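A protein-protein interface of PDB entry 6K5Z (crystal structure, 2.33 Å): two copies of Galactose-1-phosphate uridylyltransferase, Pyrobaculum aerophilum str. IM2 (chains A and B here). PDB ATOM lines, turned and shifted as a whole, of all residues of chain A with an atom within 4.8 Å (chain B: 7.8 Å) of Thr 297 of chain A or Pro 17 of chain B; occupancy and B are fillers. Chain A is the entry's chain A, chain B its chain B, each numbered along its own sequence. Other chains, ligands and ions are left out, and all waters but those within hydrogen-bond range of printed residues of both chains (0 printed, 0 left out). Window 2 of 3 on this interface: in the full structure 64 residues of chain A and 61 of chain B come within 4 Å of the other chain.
Of chain B, only Pro 17 comes within 4 Å of Thr 297 of chain A. Pro 17 of chain B touches just these residues of chain A: Asp 295 (3.3 Å) and Thr 297 (3.9 Å). Of chain B, only Arg 4 (3.4 Å) comes within 4 Å of Pro 298 of chain A. Printed residues of chain B within 4 Å of Asp 295 of chain A: Ser 16 (3.9 Å), Pro 17 (3.3 Å), His 18 (3.3 Å) and Leu 20 (3.4 Å). Printed residues of chain A within 4 Å of Leu 14 of chain B: Leu 294. Of the printed residues of chain A, Leu 20 of chain B touches Asp 295 (3.4 Å). Thr 63 of chain B touches none of the printed residues of chain A. The nearest printed residue of chain A that does not touch Ser 16 of chain B is Thr 296 of chain A (5.3 Å).
O of Pro 53 of chain B is in hydrogen-bond range of OG of Ser 16 of chain B (3.3 Å). NE of Arg 4 of chain B is in salt-bridge range of OE1 of Glu 2 of chain B. The backbone carbonyl oxygen (O) of Thr 297 of chain A sits at hydrogen-bond distance from the side-chain hydroxyl (OG1) of Thr 301 of chain A, at 3.2 Å. OG1 of Thr 297 of chain A sits at hydrogen-bond distance from N of Glu 300 of chain A (2.8 Å).
No position is printed for both chains. Of the 9 pairs that touch across the chains among the printed residues, none has its exchanged pair printed and touching as well.
Ser 16 of chain B touches Asp 295 of chain A (O to CA, 3.9 Å). Asp 295 of chain A touches Pro 17 of chain B (O to CA, 3.3 Å). CD1 of Leu 20 of chain B touches OD2 of Asp 295 of chain A, at 3.4 Å. Pro 17 of chain B touches Thr 297 of chain A (CG to CG2, 3.9 Å). Arg 4 of chain B touches Pro 298 of chain A (NH1 to CG, 3.4 Å).
Printed residues of chain A that touch a printed residue of chain B: Leu 294, Asp 295, Thr 297, Pro 298 and Glu 299. Hydrophobic or aromatic side chains of chain A within 4 Å of the printed part of chain B: Pro 298. Printed residues of chain B that touch a printed residue of chain A: Arg 4, Leu 14, Ser 16, Pro 17, His 18 and Leu 20. Hydrophobic or aromatic side chains of chain B that line the printed part of chain A: Pro 17, His 18 and Leu 20. Among the printed residues, 9 pairs touch across the chains.
O of Leu 14 of chain B is in hydrogen-bond range of N of Leu 294 of chain A (3.1 Å). N of Ser 16 of chain B is in hydrogen-bond range of O of Leu 294 of chain A, at 3.2 Å. The guanidinium group (NH2) of Arg 4 of chain B lies within salt-bridge range of the side-chain carboxylate (OE1) of Glu 299 of chain A (2.8 Å). N of His 18 of chain B sits at hydrogen-bond distance from O of Asp 295 of chain A, 3.3 Å away.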
ATOM      1  N   LEU A 294     -14.955 -27.320  -7.817  1.00  0.00           N
ATOM      2  CA  LEU A 294     -16.076 -26.493  -7.381  1.00  0.00           C
ATOM      3  C   LEU A 294     -15.676 -25.507  -6.267  1.00  0.00           C
ATOM      4  O   LEU A 294     -14.936 -25.815  -5.363  1.00  0.00           O
ATOM      5  CB  LEU A 294     -17.211 -27.368  -6.837  1.00  0.00           C
ATOM      6  CG  LEU A 294     -18.161 -28.116  -7.764  1.00  0.00           C
ATOM      7  CD1 LEU A 294     -19.107 -28.892  -6.873  1.00  0.00           C
ATOM      8  CD2 LEU A 294     -18.946 -27.183  -8.666  1.00  0.00           C
ATOM      9  N   ASP A 295     -16.210 -24.312  -6.336  1.00  0.00           N
ATOM     10  CA  ASP A 295     -15.888 -23.285  -5.379  1.00  0.00           C
ATOM     11  C   ASP A 295     -17.009 -23.165  -4.365  1.00  0.00           C
ATOM     12  O   ASP A 295     -16.910 -22.399  -3.437  1.00  0.00           O
ATOM     13  CB  ASP A 295     -15.576 -21.938  -6.105  1.00  0.00           C
ATOM     14  CG  ASP A 295     -16.615 -21.538  -7.142  1.00  0.00           C
ATOM     15  OD1 ASP A 295     -17.316 -22.383  -7.727  1.00  0.00           O
ATOM     16  OD2 ASP A 295     -16.712 -20.343  -7.399  1.00  0.00           O
ATOM     17  N   THR A 296     -18.073 -23.927  -4.555  1.00  0.00           N
ATOM     18  CA  THR A 296     -19.207 -23.943  -3.659  1.00  0.00           C
ATOM     19  C   THR A 296     -19.695 -25.397  -3.488  1.00  0.00           C
ATOM     20  O   THR A 296     -19.590 -26.211  -4.401  1.00  0.00           O
ATOM     21  CB  THR A 296     -20.269 -23.027  -4.229  1.00  0.00           C
ATOM     22  OG1 THR A 296     -19.764 -21.693  -4.204  1.00  0.00           O
ATOM     23  CG2 THR A 296     -21.553 -23.071  -3.441  1.00  0.00           C
ATOM     24  N   THR A 297     -20.180 -25.740  -2.303  1.00  0.00           N
ATOM     25  CA  THR A 297     -20.621 -27.116  -2.067  1.00  0.00           C
ATOM     26  C   THR A 297     -21.871 -27.354  -2.885  1.00  0.00           C
ATOM     27  O   THR A 297     -22.707 -26.439  -2.995  1.00  0.00           O
ATOM     28  CB  THR A 297     -21.008 -27.394  -0.597  1.00  0.00           C
ATOM     29  OG1 THR A 297     -22.033 -26.464  -0.213  1.00  0.00           O
ATOM     30  CG2 THR A 297     -19.808 -27.267   0.300  1.00  0.00           C
ATOM     31  N   PRO A 298     -22.046 -28.582  -3.384  1.00  0.00           N
ATOM     32  CA  PRO A 298     -23.341 -28.987  -3.944  1.00  0.00           C
ATOM     33  C   PRO A 298     -24.512 -28.764  -3.007  1.00  0.00           C
ATOM     34  O   PRO A 298     -25.592 -28.369  -3.451  1.00  0.00           O
ATOM     35  CB  PRO A 298     -23.151 -30.470  -4.186  1.00  0.00           C
ATOM     36  CG  PRO A 298     -21.709 -30.567  -4.529  1.00  0.00           C
ATOM     37  CD  PRO A 298     -21.062 -29.661  -3.518  1.00  0.00           C
ATOM     38  N   GLU A 299     -24.277 -28.939  -1.714  1.00  0.00           N
ATOM     39  CA  GLU A 299     -25.308 -28.680  -0.696  1.00  0.00           C
ATOM     40  C   GLU A 299     -25.769 -27.202  -0.653  1.00  0.00           C
ATOM     41  O   GLU A 299     -26.963 -26.907  -0.728  1.00  0.00           O
ATOM     42  CB  GLU A 299     -24.806 -29.185   0.661  1.00  0.00           C
ATOM     43  CG  GLU A 299     -24.624 -30.701   0.696  1.00  0.00           C
ATOM     44  CD  GLU A 299     -23.405 -31.244  -0.065  1.00  0.00           C
ATOM     45  OE1 GLU A 299     -22.324 -30.630  -0.048  1.00  0.00           O
ATOM     46  OE2 GLU A 299     -23.497 -32.333  -0.670  1.00  0.00           O
ATOM     47  N   GLU A 300     -24.829 -26.270  -0.590  1.00  0.00           N
ATOM     48  CA  GLU A 300     -25.164 -24.837  -0.560  1.00  0.00           C
ATOM     49  C   GLU A 300     -25.812 -24.448  -1.890  1.00  0.00           C
ATOM     50  O   GLU A 300     -26.853 -23.790  -1.916  1.00  0.00           O
ATOM     51  CB  GLU A 300     -23.908 -24.008  -0.253  1.00  0.00           C
ATOM     52  CG  GLU A 300     -24.132 -22.552   0.165  1.00  0.00           C
ATOM     53  CD  GLU A 300     -22.870 -21.674   0.003  1.00  0.00           C
ATOM     54  OE1 GLU A 300     -21.757 -22.145   0.343  1.00  0.00           O
ATOM     55  OE2 GLU A 300     -22.989 -20.513  -0.481  1.00  0.00           O
ATOM     56  N   THR A 301     -25.257 -24.903  -3.001  1.00  0.00           N
ATOM     57  CA  THR A 301     -25.912 -24.666  -4.312  1.00  0.00           C
ATOM     58  C   THR A 301     -27.351 -25.248  -4.412  1.00  0.00           C
ATOM     59  O   THR A 301     -28.262 -24.663  -5.031  1.00  0.00           O
ATOM     60  CB  THR A 301     -25.058 -25.215  -5.485  1.00  0.00           C
ATOM     61  OG1 THR A 301     -23.730 -24.671  -5.418  1.00  0.00           O
ATOM     62  CG2 THR A 301     -25.668 -24.827  -6.794  1.00  0.00           C
ATOM     63  N   MET B   1     -14.257 -28.923   2.277  1.00  0.00           N
ATOM     64  CA  MET B   1     -13.167 -29.354   1.352  1.00  0.00           C
ATOM     65  C   MET B   1     -12.958 -30.879   1.282  1.00  0.00           C
ATOM     66  O   MET B   1     -12.748 -31.507   2.309  1.00  0.00           O
ATOM     67  CB  MET B   1     -11.858 -28.670   1.742  1.00  0.00           C
ATOM     68  CG  MET B   1     -10.721 -28.996   0.799  1.00  0.00           C
ATOM     69  SD  MET B   1      -9.279 -27.971   1.114  1.00  0.00           S
ATOM     70  CE  MET B   1      -8.294 -28.344  -0.338  1.00  0.00           C
ATOM     71  N   GLU B   2     -12.998 -31.439   0.069  1.00  0.00           N
ATOM     72  CA  GLU B   2     -12.705 -32.860  -0.211  1.00  0.00           C
ATOM     73  C   GLU B   2     -12.738 -33.204  -1.700  1.00  0.00           C
ATOM     74  O   GLU B   2     -13.301 -32.485  -2.491  1.00  0.00           O
ATOM     75  CB  GLU B   2     -13.664 -33.823   0.517  1.00  0.00           C
ATOM     76  CG  GLU B   2     -15.124 -33.888   0.045  1.00  0.00           C
ATOM     77  CD  GLU B   2     -15.982 -32.777   0.573  1.00  0.00           C
ATOM     78  OE1 GLU B   2     -16.822 -32.259  -0.183  1.00  0.00           O
ATOM     79  OE2 GLU B   2     -15.820 -32.426   1.750  1.00  0.00           O
ATOM     80  N   ARG B   4     -14.485 -35.595  -4.050  1.00  0.00           N
ATOM     81  CA  ARG B   4     -15.651 -36.479  -4.233  1.00  0.00           C
ATOM     82  C   ARG B   4     -15.465 -37.320  -5.494  1.00  0.00           C
ATOM     83  O   ARG B   4     -14.620 -37.016  -6.321  1.00  0.00           O
ATOM     84  CB  ARG B   4     -16.962 -35.679  -4.328  1.00  0.00           C
ATOM     85  CG  ARG B   4     -17.174 -34.683  -3.197  1.00  0.00           C
ATOM     86  CD  ARG B   4     -18.609 -34.187  -3.062  1.00  0.00           C
ATOM     87  NE  ARG B   4     -18.758 -33.331  -1.903  1.00  0.00           N
ATOM     88  CZ  ARG B   4     -19.901 -32.783  -1.502  1.00  0.00           C
ATOM     89  NH1 ARG B   4     -21.014 -32.994  -2.186  1.00  0.00           N
ATOM     90  NH2 ARG B   4     -19.921 -31.957  -0.424  1.00  0.00           N
ATOM     91  N   LEU B  14     -12.916 -31.871  -7.310  1.00  0.00           N
ATOM     92  CA  LEU B  14     -12.192 -31.199  -6.258  1.00  0.00           C
ATOM     93  C   LEU B  14     -13.065 -30.133  -5.663  1.00  0.00           C
ATOM     94  O   LEU B  14     -13.037 -28.961  -6.080  1.00  0.00           O
ATOM     95  CB  LEU B  14     -10.872 -30.626  -6.788  1.00  0.00           C
ATOM     96  CG  LEU B  14     -10.025 -31.632  -7.601  1.00  0.00           C
ATOM     97  CD1 LEU B  14      -8.717 -31.015  -8.040  1.00  0.00           C
ATOM     98  CD2 LEU B  14      -9.736 -32.888  -6.830  1.00  0.00           C
ATOM     99  N   VAL B  15     -13.823 -30.525  -4.642  1.00  0.00           N
ATOM    100  CA  VAL B  15     -14.677 -29.594  -3.920  1.00  0.00           C
ATOM    101  C   VAL B  15     -13.780 -28.870  -2.903  1.00  0.00           C
ATOM    102  O   VAL B  15     -13.186 -29.507  -2.033  1.00  0.00           O
ATOM    103  CB  VAL B  15     -15.857 -30.312  -3.229  1.00  0.00           C
ATOM    104  CG1 VAL B  15     -16.824 -29.308  -2.561  1.00  0.00           C
ATOM    105  CG2 VAL B  15     -16.614 -31.167  -4.230  1.00  0.00           C
ATOM    106  N   SER B  16     -13.631 -27.555  -3.058  1.00  0.00           N
ATOM    107  CA  SER B  16     -12.835 -26.743  -2.133  1.00  0.00           C
ATOM    108  C   SER B  16     -13.441 -25.372  -2.176  1.00  0.00           C
ATOM    109  O   SER B  16     -13.080 -24.567  -3.037  1.00  0.00           O
ATOM    110  CB  SER B  16     -11.318 -26.719  -2.446  1.00  0.00           C
ATOM    111  OG  SER B  16     -11.016 -26.060  -3.649  1.00  0.00           O
ATOM    112  N   PRO B  17     -14.404 -25.127  -1.260  1.00  0.00           N
ATOM    113  CA  PRO B  17     -15.077 -23.854  -1.118  1.00  0.00           C
ATOM    114  C   PRO B  17     -14.163 -22.693  -0.748  1.00  0.00           C
ATOM    115  O   PRO B  17     -13.317 -22.812   0.144  1.00  0.00           O
ATOM    116  CB  PRO B  17     -16.083 -24.099   0.026  1.00  0.00           C
ATOM    117  CG  PRO B  17     -16.317 -25.551   0.022  1.00  0.00           C
ATOM    118  CD  PRO B  17     -14.996 -26.145  -0.372  1.00  0.00           C
ATOM    119  N   HIS B  18     -14.342 -21.590  -1.460  1.00  0.00           N
ATOM    120  CA  HIS B  18     -13.839 -20.308  -1.023  1.00  0.00           C
ATOM    121  C   HIS B  18     -14.886 -19.252  -1.367  1.00  0.00           C
ATOM    122  O   HIS B  18     -15.640 -19.396  -2.316  1.00  0.00           O
ATOM    123  CB  HIS B  18     -12.442 -20.007  -1.617  1.00  0.00           C
ATOM    124  CG  HIS B  18     -12.378 -20.035  -3.106  1.00  0.00           C
ATOM    125  ND1 HIS B  18     -12.723 -18.946  -3.883  1.00  0.00           N
ATOM    126  CD2 HIS B  18     -11.961 -20.997  -3.966  1.00  0.00           C
ATOM    127  CE1 HIS B  18     -12.537 -19.242  -5.159  1.00  0.00           C
ATOM    128  NE2 HIS B  18     -12.079 -20.482  -5.238  1.00  0.00           N
ATOM    129  N   ARG B  19     -14.932 -18.189  -0.575  1.00  0.00           N
ATOM    130  CA  ARG B  19     -15.887 -17.129  -0.837  1.00  0.00           C
ATOM    131  C   ARG B  19     -15.525 -16.512  -2.180  1.00  0.00           C
ATOM    132  O   ARG B  19     -14.349 -16.335  -2.492  1.00  0.00           O
ATOM    133  CB  ARG B  19     -15.849 -16.083   0.275  1.00  0.00           C
ATOM    134  CG  ARG B  19     -17.143 -15.303   0.432  1.00  0.00           C
ATOM    135  CD  ARG B  19     -17.029 -14.265   1.535  1.00  0.00           C
ATOM    136  NE  ARG B  19     -18.221 -13.425   1.617  1.00  0.00           N
ATOM    137  CZ  ARG B  19     -18.502 -12.449   0.762  1.00  0.00           C
ATOM    138  NH1 ARG B  19     -17.683 -12.190  -0.246  1.00  0.00           N
ATOM    139  NH2 ARG B  19     -19.607 -11.733   0.913  1.00  0.00           N
ATOM    140  N   LEU B  20     -16.535 -16.185  -2.975  1.00  0.00           N
ATOM    141  CA  LEU B  20     -16.304 -15.610  -4.292  1.00  0.00           C
ATOM    142  C   LEU B  20     -16.387 -14.092  -4.218  1.00  0.00           C
ATOM    143  O   LEU B  20     -17.306 -13.539  -3.616  1.00  0.00           O
ATOM    144  CB  LEU B  20     -17.309 -16.165  -5.303  1.00  0.00           C
ATOM    145  CG  LEU B  20     -16.847 -16.270  -6.759  1.00  0.00           C
ATOM    146  CD1 LEU B  20     -17.784 -17.163  -7.558  1.00  0.00           C
ATOM    147  CD2 LEU B  20     -16.721 -14.901  -7.410  1.00  0.00           C
ATOM    148  N   TYR B  52      -6.073 -19.977  -3.736  1.00  0.00           N
ATOM    149  CA  TYR B  52      -7.281 -20.739  -3.424  1.00  0.00           C
ATOM    150  C   TYR B  52      -7.001 -22.202  -3.792  1.00  0.00           C
ATOM    151  O   TYR B  52      -7.371 -22.661  -4.879  1.00  0.00           O
ATOM    152  CB  TYR B  52      -8.444 -20.163  -4.228  1.00  0.00           C
ATOM    153  CG  TYR B  52      -8.662 -18.700  -3.897  1.00  0.00           C
ATOM    154  CD1 TYR B  52      -9.266 -18.318  -2.687  1.00  0.00           C
ATOM    155  CD2 TYR B  52      -8.223 -17.689  -4.766  1.00  0.00           C
ATOM    156  CE1 TYR B  52      -9.448 -16.984  -2.361  1.00  0.00           C
ATOM    157  CE2 TYR B  52      -8.399 -16.348  -4.440  1.00  0.00           C
ATOM    158  CZ  TYR B  52      -8.999 -16.008  -3.233  1.00  0.00           C
ATOM    159  OH  TYR B  52      -9.173 -14.687  -2.912  1.00  0.00           O
ATOM    160  N   PRO B  53      -6.294 -22.933  -2.911  1.00  0.00           N
ATOM    161  CA  PRO B  53      -5.874 -24.280  -3.332  1.00  0.00           C
ATOM    162  C   PRO B  53      -7.035 -25.301  -3.385  1.00  0.00           C
ATOM    163  O   PRO B  53      -7.997 -25.224  -2.588  1.00  0.00           O
ATOM    164  CB  PRO B  53      -4.800 -24.681  -2.293  1.00  0.00           C
ATOM    165  CG  PRO B  53      -4.672 -23.526  -1.338  1.00  0.00           C
ATOM    166  CD  PRO B  53      -5.815 -22.589  -1.556  1.00  0.00           C
ATOM    167  N   VAL B  54      -6.942 -26.223  -4.334  1.00  0.00           N
ATOM    168  CA  VAL B  54      -7.973 -27.268  -4.508  1.00  0.00           C
ATOM    169  C   VAL B  54      -7.582 -28.570  -3.827  1.00  0.00           C
ATOM    170  O   VAL B  54      -8.427 -29.372  -3.469  1.00  0.00           O
ATOM    171  CB  VAL B  54      -8.353 -27.489  -5.996  1.00  0.00           C
ATOM    172  CG1 VAL B  54      -8.980 -26.211  -6.552  1.00  0.00           C
ATOM    173  CG2 VAL B  54      -7.171 -27.967  -6.838  1.00  0.00           C
ATOM    174  N   THR B  63     -16.050 -34.470   3.921  1.00  0.00           N
ATOM    175  CA  THR B  63     -17.507 -34.685   3.985  1.00  0.00           C
ATOM    176  C   THR B  63     -17.833 -36.067   3.442  1.00  0.00           C
ATOM    177  O   THR B  63     -17.371 -36.424   2.361  1.00  0.00           O
ATOM    178  CB  THR B  63     -18.263 -33.654   3.124  1.00  0.00           C
ATOM    179  OG1 THR B  63     -17.835 -32.327   3.474  1.00  0.00           O
ATOM    180  CG2 THR B  63     -19.785 -33.765   3.309  1.00  0.00           C
